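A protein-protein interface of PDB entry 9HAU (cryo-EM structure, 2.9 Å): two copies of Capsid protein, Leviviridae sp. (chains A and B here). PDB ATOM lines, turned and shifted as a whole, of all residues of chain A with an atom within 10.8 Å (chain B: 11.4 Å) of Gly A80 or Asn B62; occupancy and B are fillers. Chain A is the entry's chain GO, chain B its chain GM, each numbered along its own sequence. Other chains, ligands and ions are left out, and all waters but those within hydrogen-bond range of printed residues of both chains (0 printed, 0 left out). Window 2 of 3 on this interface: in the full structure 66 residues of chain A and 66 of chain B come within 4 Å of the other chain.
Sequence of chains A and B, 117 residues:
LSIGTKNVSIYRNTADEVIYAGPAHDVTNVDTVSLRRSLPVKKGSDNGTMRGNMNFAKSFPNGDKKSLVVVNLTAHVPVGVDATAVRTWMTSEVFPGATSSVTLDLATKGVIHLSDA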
ATOM      1  N   PRO A  40      15.709 -36.197  -4.373  1.00  0.00           N
ATOM      2  CA  PRO A  40      16.231 -36.076  -3.002  1.00  0.00           C
ATOM      3  C   PRO A  40      15.282 -36.680  -1.980  1.00  0.00           C
ATOM      4  O   PRO A  40      14.063 -36.511  -2.059  1.00  0.00           O
ATOM      5  CB  PRO A  40      16.375 -34.563  -2.813  1.00  0.00           C
ATOM      6  CG  PRO A  40      16.417 -33.996  -4.187  1.00  0.00           C
ATOM      7  CD  PRO A  40      15.593 -34.893  -5.046  1.00  0.00           C
ATOM      8  N   LYS A  42      14.440 -36.501   1.903  1.00  0.00           N
ATOM      9  CA  LYS A  42      14.624 -35.697   3.110  1.00  0.00           C
ATOM     10  C   LYS A  42      14.704 -36.654   4.293  1.00  0.00           C
ATOM     11  O   LYS A  42      13.688 -37.072   4.851  1.00  0.00           O
ATOM     12  CB  LYS A  42      13.487 -34.692   3.294  1.00  0.00           C
ATOM     13  CG  LYS A  42      12.683 -34.258   2.046  1.00  0.00           C
ATOM     14  CD  LYS A  42      13.526 -33.864   0.831  1.00  0.00           C
ATOM     15  CE  LYS A  42      14.009 -32.426   0.943  1.00  0.00           C
ATOM     16  NZ  LYS A  42      14.289 -31.826  -0.390  1.00  0.00           N
ATOM     17  N   SER A  45      18.234 -34.510   9.418  1.00  0.00           N
ATOM     18  CA  SER A  45      18.437 -33.091   9.158  1.00  0.00           C
ATOM     19  C   SER A  45      18.999 -32.827   7.769  1.00  0.00           C
ATOM     20  O   SER A  45      19.101 -31.663   7.367  1.00  0.00           O
ATOM     21  CB  SER A  45      19.372 -32.486  10.210  1.00  0.00           C
ATOM     22  OG  SER A  45      20.699 -32.390   9.719  1.00  0.00           O
ATOM     23  N   ASP A  46      19.364 -33.874   7.035  1.00  0.00           N
ATOM     24  CA  ASP A  46      19.878 -33.719   5.683  1.00  0.00           C
ATOM     25  C   ASP A  46      18.723 -33.674   4.692  1.00  0.00           C
ATOM     26  O   ASP A  46      17.872 -34.569   4.672  1.00  0.00           O
ATOM     27  CB  ASP A  46      20.829 -34.862   5.339  1.00  0.00           C
ATOM     28  CG  ASP A  46      21.258 -34.846   3.889  1.00  0.00           C
ATOM     29  OD1 ASP A  46      21.166 -35.900   3.228  1.00  0.00           O
ATOM     30  OD2 ASP A  46      21.688 -33.777   3.408  1.00  0.00           O
ATOM     31  N   ASN A  47      18.692 -32.630   3.872  1.00  0.00           N
ATOM     32  CA  ASN A  47      17.636 -32.473   2.883  1.00  0.00           C
ATOM     33  C   ASN A  47      17.790 -33.413   1.695  1.00  0.00           C
ATOM     34  O   ASN A  47      16.889 -33.475   0.855  1.00  0.00           O
ATOM     35  CB  ASN A  47      17.582 -31.023   2.404  1.00  0.00           C
ATOM     36  CG  ASN A  47      16.924 -30.106   3.412  1.00  0.00           C
ATOM     37  OD1 ASN A  47      15.952 -30.479   4.064  1.00  0.00           O
ATOM     38  ND2 ASN A  47      17.452 -28.896   3.546  1.00  0.00           N
ATOM     39  N   GLY A  48      18.893 -34.139   1.599  1.00  0.00           N
ATOM     40  CA  GLY A  48      19.082 -35.100   0.534  1.00  0.00           C
ATOM     41  C   GLY A  48      19.893 -34.545  -0.617  1.00  0.00           C
ATOM     42  O   GLY A  48      20.427 -33.433  -0.583  1.00  0.00           O
ATOM     43  N   THR A  49      19.981 -35.358  -1.665  1.00  0.00           N
ATOM     44  CA  THR A  49      20.796 -35.045  -2.829  1.00  0.00           C
ATOM     45  C   THR A  49      20.056 -35.471  -4.086  1.00  0.00           C
ATOM     46  O   THR A  49      19.467 -36.554  -4.125  1.00  0.00           O
ATOM     47  CB  THR A  49      22.157 -35.750  -2.753  1.00  0.00           C
ATOM     48  OG1 THR A  49      22.806 -35.404  -1.524  1.00  0.00           O
ATOM     49  CG2 THR A  49      23.044 -35.345  -3.914  1.00  0.00           C
ATOM     50  N   MET A  50      20.087 -34.620  -5.106  1.00  0.00           N
ATOM     51  CA  MET A  50      19.536 -34.953  -6.412  1.00  0.00           C
ATOM     52  C   MET A  50      20.620 -35.610  -7.256  1.00  0.00           C
ATOM     53  O   MET A  50      21.689 -35.029  -7.464  1.00  0.00           O
ATOM     54  CB  MET A  50      18.996 -33.705  -7.109  1.00  0.00           C
ATOM     55  CG  MET A  50      18.536 -33.944  -8.541  1.00  0.00           C
ATOM     56  SD  MET A  50      16.800 -34.409  -8.668  1.00  0.00           S
ATOM     57  CE  MET A  50      16.003 -32.855  -8.271  1.00  0.00           C
ATOM     58  N   HIS A  76      25.869 -35.145  -8.584  1.00  0.00           N
ATOM     59  CA  HIS A  76      25.302 -35.235  -7.243  1.00  0.00           C
ATOM     60  C   HIS A  76      25.227 -33.829  -6.665  1.00  0.00           C
ATOM     61  O   HIS A  76      26.244 -33.279  -6.230  1.00  0.00           O
ATOM     62  CB  HIS A  76      26.135 -36.150  -6.347  1.00  0.00           C
ATOM     63  CG  HIS A  76      26.373 -37.511  -6.922  1.00  0.00           C
ATOM     64  ND1 HIS A  76      25.874 -38.658  -6.345  1.00  0.00           N
ATOM     65  CD2 HIS A  76      27.071 -37.911  -8.012  1.00  0.00           C
ATOM     66  CE1 HIS A  76      26.246 -39.705  -7.059  1.00  0.00           C
ATOM     67  NE2 HIS A  76      26.973 -39.279  -8.076  1.00  0.00           N
ATOM     68  N   VAL A  77      24.032 -33.250  -6.660  1.00  0.00           N
ATOM     69  CA  VAL A  77      23.816 -31.883  -6.207  1.00  0.00           C
ATOM     70  C   VAL A  77      22.996 -31.924  -4.923  1.00  0.00           C
ATOM     71  O   VAL A  77      21.814 -32.275  -4.957  1.00  0.00           O
ATOM     72  CB  VAL A  77      23.114 -31.028  -7.274  1.00  0.00           C
ATOM     73  CG1 VAL A  77      23.184 -29.560  -6.902  1.00  0.00           C
ATOM     74  CG2 VAL A  77      23.743 -31.267  -8.635  1.00  0.00           C
ATOM     75  N   PRO A  78      23.573 -31.586  -3.772  1.00  0.00           N
ATOM     76  CA  PRO A  78      22.789 -31.569  -2.530  1.00  0.00           C
ATOM     77  C   PRO A  78      21.761 -30.449  -2.530  1.00  0.00           C
ATOM     78  O   PRO A  78      21.974 -29.382  -3.108  1.00  0.00           O
ATOM     79  CB  PRO A  78      23.847 -31.357  -1.439  1.00  0.00           C
ATOM     80  CG  PRO A  78      25.171 -31.599  -2.106  1.00  0.00           C
ATOM     81  CD  PRO A  78      24.984 -31.243  -3.539  1.00  0.00           C
ATOM     82  N   VAL A  79      20.631 -30.707  -1.866  1.00  0.00           N
ATOM     83  CA  VAL A  79      19.590 -29.694  -1.741  1.00  0.00           C
ATOM     84  C   VAL A  79      20.097 -28.541  -0.887  1.00  0.00           C
ATOM     85  O   VAL A  79      20.726 -28.742   0.159  1.00  0.00           O
ATOM     86  CB  VAL A  79      18.313 -30.310  -1.145  1.00  0.00           C
ATOM     87  CG1 VAL A  79      17.272 -29.235  -0.874  1.00  0.00           C
ATOM     88  CG2 VAL A  79      17.756 -31.361  -2.075  1.00  0.00           C
ATOM     89  N   GLY A  80      19.824 -27.318  -1.337  1.00  0.00           N
ATOM     90  CA  GLY A  80      20.236 -26.114  -0.652  1.00  0.00           C
ATOM     91  C   GLY A  80      21.316 -25.332  -1.365  1.00  0.00           C
ATOM     92  O   GLY A  80      21.605 -24.198  -0.970  1.00  0.00           O
ATOM     93  N   VAL A  81      21.913 -25.904  -2.398  1.00  0.00           N
ATOM     94  CA  VAL A  81      22.960 -25.234  -3.155  1.00  0.00           C
ATOM     95  C   VAL A  81      22.327 -24.364  -4.235  1.00  0.00           C
ATOM     96  O   VAL A  81      21.263 -24.681  -4.776  1.00  0.00           O
ATOM     97  CB  VAL A  81      23.929 -26.276  -3.750  1.00  0.00           C
ATOM     98  CG1 VAL A  81      24.997 -25.613  -4.588  1.00  0.00           C
ATOM     99  CG2 VAL A  81      24.562 -27.093  -2.639  1.00  0.00           C
ATOM    100  N   ASP A  82      22.980 -23.247  -4.542  1.00  0.00           N
ATOM    101  CA  ASP A  82      22.515 -22.375  -5.610  1.00  0.00           C
ATOM    102  C   ASP A  82      22.639 -23.085  -6.952  1.00  0.00           C
ATOM    103  O   ASP A  82      23.726 -23.524  -7.338  1.00  0.00           O
ATOM    104  CB  ASP A  82      23.321 -21.077  -5.615  1.00  0.00           C
ATOM    105  CG  ASP A  82      22.791 -20.062  -6.606  1.00  0.00           C
ATOM    106  OD1 ASP A  82      23.470 -19.037  -6.821  1.00  0.00           O
ATOM    107  OD2 ASP A  82      21.694 -20.277  -7.161  1.00  0.00           O
ATOM    108  N   ALA A  83      21.517 -23.199  -7.666  1.00  0.00           N
ATOM    109  CA  ALA A  83      21.517 -23.914  -8.938  1.00  0.00           C
ATOM    110  C   ALA A  83      22.281 -23.155 -10.015  1.00  0.00           C
ATOM    111  O   ALA A  83      22.937 -23.776 -10.857  1.00  0.00           O
ATOM    112  CB  ALA A  83      20.083 -24.183  -9.391  1.00  0.00           C
ATOM    113  N   THR A  84      22.200 -21.824 -10.013  1.00  0.00           N
ATOM    114  CA  THR A  84      22.947 -21.035 -10.988  1.00  0.00           C
ATOM    115  C   THR A  84      24.449 -21.174 -10.776  1.00  0.00           C
ATOM    116  O   THR A  84      25.215 -21.237 -11.746  1.00  0.00           O
ATOM    117  CB  THR A  84      22.531 -19.567 -10.907  1.00  0.00           C
ATOM    118  OG1 THR A  84      21.102 -19.471 -10.947  1.00  0.00           O
ATOM    119  CG2 THR A  84      23.117 -18.781 -12.068  1.00  0.00           C
ATOM    120  N   ALA A  85      24.889 -21.217  -9.518  1.00  0.00           N
ATOM    121  CA  ALA A  85      26.310 -21.387  -9.233  1.00  0.00           C
ATOM    122  C   ALA A  85      26.821 -22.728  -9.745  1.00  0.00           C
ATOM    123  O   ALA A  85      27.927 -22.813 -10.288  1.00  0.00           O
ATOM    124  CB  ALA A  85      26.563 -21.251  -7.733  1.00  0.00           C
ATOM    125  N   VAL A  86      26.031 -23.790  -9.574  1.00  0.00           N
ATOM    126  CA  VAL A  86      26.450 -25.109 -10.040  1.00  0.00           C
ATOM    127  C   VAL A  86      26.500 -25.150 -11.563  1.00  0.00           C
ATOM    128  O   VAL A  86      27.426 -25.719 -12.151  1.00  0.00           O
ATOM    129  CB  VAL A  86      25.522 -26.196  -9.472  1.00  0.00           C
ATOM    130  CG1 VAL A  86      25.757 -27.523 -10.174  1.00  0.00           C
ATOM    131  CG2 VAL A  86      25.742 -26.345  -7.985  1.00  0.00           C
ATOM    132  N   THR B  28      39.834 -25.713   3.514  1.00  0.00           N
ATOM    133  CA  THR B  28      38.429 -25.369   3.677  1.00  0.00           C
ATOM    134  C   THR B  28      37.594 -25.560   2.418  1.00  0.00           C
ATOM    135  O   THR B  28      36.403 -25.866   2.528  1.00  0.00           O
ATOM    136  CB  THR B  28      38.295 -23.912   4.152  1.00  0.00           C
ATOM    137  OG1 THR B  28      39.107 -23.716   5.315  1.00  0.00           O
ATOM    138  CG2 THR B  28      36.855 -23.578   4.502  1.00  0.00           C
ATOM    139  N   ASN B  29      38.183 -25.422   1.234  1.00  0.00           N
ATOM    140  CA  ASN B  29      37.436 -25.480  -0.015  1.00  0.00           C
ATOM    141  C   ASN B  29      37.946 -26.631  -0.866  1.00  0.00           C
ATOM    142  O   ASN B  29      39.159 -26.825  -0.992  1.00  0.00           O
ATOM    143  CB  ASN B  29      37.548 -24.162  -0.783  1.00  0.00           C
ATOM    144  CG  ASN B  29      37.134 -22.969   0.050  1.00  0.00           C
ATOM    145  OD1 ASN B  29      35.947 -22.722   0.252  1.00  0.00           O
ATOM    146  ND2 ASN B  29      38.113 -22.224   0.544  1.00  0.00           N
ATOM    147  N   LYS B  58      33.581 -30.071  -6.083  1.00  0.00           N
ATOM    148  CA  LYS B  58      33.647 -28.658  -5.743  1.00  0.00           C
ATOM    149  C   LYS B  58      32.731 -28.379  -4.562  1.00  0.00           C
ATOM    150  O   LYS B  58      31.553 -28.745  -4.589  1.00  0.00           O
ATOM    151  CB  LYS B  58      33.253 -27.786  -6.938  1.00  0.00           C
ATOM    152  CG  LYS B  58      33.244 -26.300  -6.649  1.00  0.00           C
ATOM    153  CD  LYS B  58      34.584 -25.668  -6.955  1.00  0.00           C
ATOM    154  CE  LYS B  58      34.518 -24.162  -6.794  1.00  0.00           C
ATOM    155  NZ  LYS B  58      35.818 -23.594  -6.354  1.00  0.00           N
ATOM    156  N   SER B  59      33.274 -27.737  -3.535  1.00  0.00           N
ATOM    157  CA  SER B  59      32.466 -27.305  -2.405  1.00  0.00           C
ATOM    158  C   SER B  59      31.672 -26.058  -2.770  1.00  0.00           C
ATOM    159  O   SER B  59      32.154 -25.169  -3.477  1.00  0.00           O
ATOM    160  CB  SER B  59      33.348 -27.036  -1.185  1.00  0.00           C
ATOM    161  OG  SER B  59      34.259 -25.982  -1.434  1.00  0.00           O
ATOM    162  N   PHE B  60      30.435 -26.004  -2.291  1.00  0.00           N
ATOM    163  CA  PHE B  60      29.532 -24.904  -2.588  1.00  0.00           C
ATOM    164  C   PHE B  60      28.881 -24.418  -1.304  1.00  0.00           C
ATOM    165  O   PHE B  60      28.698 -25.198  -0.362  1.00  0.00           O
ATOM    166  CB  PHE B  60      28.441 -25.324  -3.586  1.00  0.00           C
ATOM    167  CG  PHE B  60      28.858 -25.215  -5.021  1.00  0.00           C
ATOM    168  CD1 PHE B  60      28.689 -24.031  -5.718  1.00  0.00           C
ATOM    169  CD2 PHE B  60      29.418 -26.298  -5.677  1.00  0.00           C
ATOM    170  CE1 PHE B  60      29.072 -23.930  -7.039  1.00  0.00           C
ATOM    171  CE2 PHE B  60      29.801 -26.202  -6.997  1.00  0.00           C
ATOM    172  CZ  PHE B  60      29.630 -25.016  -7.678  1.00  0.00           C
ATOM    173  N   PRO B  61      28.529 -23.134  -1.235  1.00  0.00           N
ATOM    174  CA  PRO B  61      27.794 -22.632  -0.066  1.00  0.00           C
ATOM    175  C   PRO B  61      26.396 -23.232  -0.009  1.00  0.00           C
ATOM    176  O   PRO B  61      25.641 -23.177  -0.982  1.00  0.00           O
ATOM    177  CB  PRO B  61      27.747 -21.116  -0.291  1.00  0.00           C
ATOM    178  CG  PRO B  61      28.782 -20.830  -1.319  1.00  0.00           C
ATOM    179  CD  PRO B  61      28.922 -22.055  -2.156  1.00  0.00           C
ATOM    180  N   ASN B  62      26.060 -23.813   1.141  1.00  0.00           N
ATOM    181  CA  ASN B  62      24.744 -24.415   1.368  1.00  0.00           C
ATOM    182  C   ASN B  62      24.269 -23.928   2.735  1.00  0.00           C
ATOM    183  O   ASN B  62      24.493 -24.589   3.753  1.00  0.00           O
ATOM    184  CB  ASN B  62      24.812 -25.936   1.292  1.00  0.00           C
ATOM    185  CG  ASN B  62      23.451 -26.595   1.412  1.00  0.00           C
ATOM    186  OD1 ASN B  62      22.446 -25.938   1.671  1.00  0.00           O
ATOM    187  ND2 ASN B  62      23.416 -27.906   1.220  1.00  0.00           N
ATOM    188  N   GLY B  63      23.598 -22.786   2.746  1.00  0.00           N
ATOM    189  CA  GLY B  63      23.205 -22.182   4.006  1.00  0.00           C
ATOM    190  C   GLY B  63      24.434 -21.784   4.797  1.00  0.00           C
ATOM    191  O   GLY B  63      25.328 -21.092   4.295  1.00  0.00           O
ATOM    192  N   ASP B  64      24.495 -22.225   6.052  1.00  0.00           N
ATOM    193  CA  ASP B  64      25.643 -21.945   6.901  1.00  0.00           C
ATOM    194  C   ASP B  64      26.803 -22.902   6.671  1.00  0.00           C
ATOM    195  O   ASP B  64      27.954 -22.531   6.928  1.00  0.00           O
ATOM    196  CB  ASP B  64      25.232 -21.992   8.376  1.00  0.00           C
ATOM    197  CG  ASP B  64      24.452 -23.244   8.725  1.00  0.00           C
ATOM    198  OD1 ASP B  64      25.047 -24.342   8.716  1.00  0.00           O
ATOM    199  OD2 ASP B  64      23.240 -23.132   9.007  1.00  0.00           O
ATOM    200  N   LYS B  65      26.532 -24.112   6.197  1.00  0.00           N
ATOM    201  CA  LYS B  65      27.551 -25.121   5.981  1.00  0.00           C
ATOM    202  C   LYS B  65      28.007 -25.104   4.522  1.00  0.00           C
ATOM    203  O   LYS B  65      27.676 -24.199   3.750  1.00  0.00           O
ATOM    204  CB  LYS B  65      27.021 -26.495   6.392  1.00  0.00           C
ATOM    205  CG  LYS B  65      25.808 -26.950   5.601  1.00  0.00           C
ATOM    206  CD  LYS B  65      25.294 -28.291   6.095  1.00  0.00           C
ATOM    207  CE  LYS B  65      25.217 -29.299   4.962  1.00  0.00           C
ATOM    208  NZ  LYS B  65      26.569 -29.767   4.544  1.00  0.00           N
ATOM    209  N   LYS B  66      28.787 -26.111   4.142  1.00  0.00           N
ATOM    210  CA  LYS B  66      29.271 -26.274   2.780  1.00  0.00           C
ATOM    211  C   LYS B  66      28.864 -27.646   2.265  1.00  0.00           C
ATOM    212  O   LYS B  66      28.826 -28.619   3.023  1.00  0.00           O
ATOM    213  CB  LYS B  66      30.791 -26.117   2.708  1.00  0.00           C
ATOM    214  CG  LYS B  66      31.262 -24.679   2.638  1.00  0.00           C
ATOM    215  CD  LYS B  66      32.779 -24.599   2.637  1.00  0.00           C
ATOM    216  CE  LYS B  66      33.256 -23.159   2.689  1.00  0.00           C
ATOM    217  NZ  LYS B  66      33.283 -22.638   4.083  1.00  0.00           N
ATOM    218  N   SER B  67      28.558 -27.721   0.975  1.00  0.00           N
ATOM    219  CA  SER B  67      28.100 -28.951   0.350  1.00  0.00           C
ATOM    220  C   SER B  67      28.994 -29.297  -0.831  1.00  0.00           C
ATOM    221  O   SER B  67      29.459 -28.411  -1.552  1.00  0.00           O
ATOM    222  CB  SER B  67      26.647 -28.826  -0.110  1.00  0.00           C
ATOM    223  OG  SER B  67      25.756 -29.064   0.964  1.00  0.00           O
ATOM    224  N   LEU B  68      29.226 -30.591  -1.022  1.00  0.00           N
ATOM    225  CA  LEU B  68      30.075 -31.079  -2.100  1.00  0.00           C
ATOM    226  C   LEU B  68      29.217 -31.467  -3.296  1.00  0.00           C
ATOM    227  O   LEU B  68      28.339 -32.330  -3.185  1.00  0.00           O
ATOM    228  CB  LEU B  68      30.906 -32.271  -1.631  1.00  0.00           C
ATOM    229  CG  LEU B  68      32.170 -32.549  -2.440  1.00  0.00           C
ATOM    230  CD1 LEU B  68      33.148 -31.399  -2.301  1.00  0.00           C
ATOM    231  CD2 LEU B  68      32.804 -33.854  -1.997  1.00  0.00           C
ATOM    232  N   VAL B  69      29.476 -30.838  -4.437  1.00  0.00           N
ATOM    233  CA  VAL B  69      28.850 -31.197  -5.702  1.00  0.00           C
ATOM    234  C   VAL B  69      29.848 -32.019  -6.504  1.00  0.00           C
ATOM    235  O   VAL B  69      30.976 -31.574  -6.746  1.00  0.00           O
ATOM    236  CB  VAL B  69      28.401 -29.948  -6.481  1.00  0.00           C
ATOM    237  CG1 VAL B  69      27.894 -30.335  -7.857  1.00  0.00           C
ATOM    238  CG2 VAL B  69      27.333 -29.197  -5.706  1.00  0.00           C
ATOM    239  N   ALA B 107      21.034 -32.113 -14.050  1.00  0.00           N
ATOM    240  CA  ALA B 107      21.812 -32.064 -12.817  1.00  0.00           C
ATOM    241  C   ALA B 107      21.179 -31.140 -11.783  1.00  0.00           C
ATOM    242  O   ALA B 107      21.110 -31.483 -10.598  1.00  0.00           O
ATOM    243  CB  ALA B 107      23.243 -31.625 -13.122  1.00  0.00           C
ATOM    244  N   THR B 108      20.708 -29.969 -12.209  1.00  0.00           N
ATOM    245  CA  THR B 108      20.241 -28.949 -11.281  1.00  0.00           C
ATOM    246  C   THR B 108      18.725 -28.900 -11.133  1.00  0.00           C
ATOM    247  O   THR B 108      18.235 -28.293 -10.176  1.00  0.00           O
ATOM    248  CB  THR B 108      20.746 -27.569 -11.715  1.00  0.00           C
ATOM    249  OG1 THR B 108      20.490 -27.382 -13.111  1.00  0.00           O
ATOM    250  CG2 THR B 108      22.238 -27.449 -11.463  1.00  0.00           C
ATOM    251  N   LYS B 109      17.972 -29.511 -12.048  1.00  0.00           N
ATOM    252  CA  LYS B 109      16.521 -29.505 -11.961  1.00  0.00           C
ATOM    253  C   LYS B 109      15.900 -30.891 -12.052  1.00  0.00           C
ATOM    254  O   LYS B 109      14.691 -31.019 -11.843  1.00  0.00           O
ATOM    255  CB  LYS B 109      15.916 -28.616 -13.057  1.00  0.00           C
ATOM    256  CG  LYS B 109      16.561 -27.251 -13.185  1.00  0.00           C
ATOM    257  CD  LYS B 109      16.193 -26.599 -14.500  1.00  0.00           C
ATOM    258  CE  LYS B 109      16.040 -25.099 -14.347  1.00  0.00           C
ATOM    259  NZ  LYS B 109      16.332 -24.381 -15.614  1.00  0.00           N
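Gly A80 touches just one residue of chain B: Asn B62. Printed residues of chain A within 4 Å of Asn B62: Val A79 (3.0 Å) and Gly A80 (3.2 Å). Val A79 touches just one residue of chain B: Asn B62 (3.0 Å). Lys B65 touches none of the printed residues of chain A. Ser B67 touches just these residues of chain A: Pro A78 (3.7 Å) and Val A81 (3.7 Å). Of the printed residues of chain B, Val A81 touches Phe B60 (3.6 Å) and Ser B67 (3.7 Å). Of the printed residues of chain B, His A76 touches Leu B68 (3.8 Å) and Val B69 (3.4 Å). Lys B66 touches none of the printed residues of chain A. The nearest printed residue of chain B that does not touch Val A77 is Val B69 (4.3 Å).
The backbone carbonyl oxygen (O) of Lys B58 sits at hydrogen-bond distance from the backbone NH (N) of Val B69, at 3.0 Å. The backbone carbonyl oxygen of Ser B67 sits at hydrogen-bond distance from the backbone NH of Phe B60 (2.7 Å). ND2 of Asn B62 lies within hydrogen-bond range of OG of Ser B67 (2.6 Å). The backbone NH (N) of Val A79 sits at hydrogen-bond distance from the backbone carbonyl oxygen (O) of Gly A48, at 3.0 Å. The backbone NH (N) of Met A50 is in hydrogen-bond range of the backbone carbonyl oxygen (O) of Val A77.
No position is printed for both chains. Of the 15 pairs that touch across the chains among the printed residues, none has its exchanged pair printed and touching as well.
Among the printed residues, pairs that only touch across the chains: Val A77 with Ala B107 (3.3 Å), His A76 with Val B69 (3.4 Å), Pro A78 with Leu B68 (3.4 Å), Val A81 with Phe B60 (3.6 Å), Ala A85 with Phe B60 (3.6 Å), Val A81 with Ser B67 (3.7 Å), Pro A78 with Ser B67 (3.7 Å), Val A86 with Thr B108 (3.7 Å), Ala A83 with Thr B108 (3.8 Å), Pro A78 with Val B69 (3.8 Å), His A76 with Leu B68 (3.8 Å), Val A86 with Phe B60 (3.96 Å) and Val A86 with Val B69 (3.98 Å).
The side-chain amide nitrogen (ND2) of Asn B62 is in hydrogen-bond range of the backbone carbonyl oxygen (O) of Val A79. The side-chain amide oxygen (OD1) of Asn B62 lies close to the backbone carbonyl oxygen (O) of Gly A80, at 3.3 Å.
Hydrophobic or aromatic side chains of chain B that line the printed part of chain A: Phe B60 and Val B69. Along chain B the printed residues that touch a printed residue of chain A span positions 60 to 108. Of the 19 printed residues of chain A, 9 touch a printed residue of chain B. Printed residues of chain A that touch a printed residue of chain B: His A76, Val A77, Pro A78, Val A79, Gly A80, Val A81, Ala A83, Ala A85 and Val A86. Along chain A the printed residues that touch a printed residue of chain B span positions 76 to 86. Among the printed residues, 15 pairs touch across the chains.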
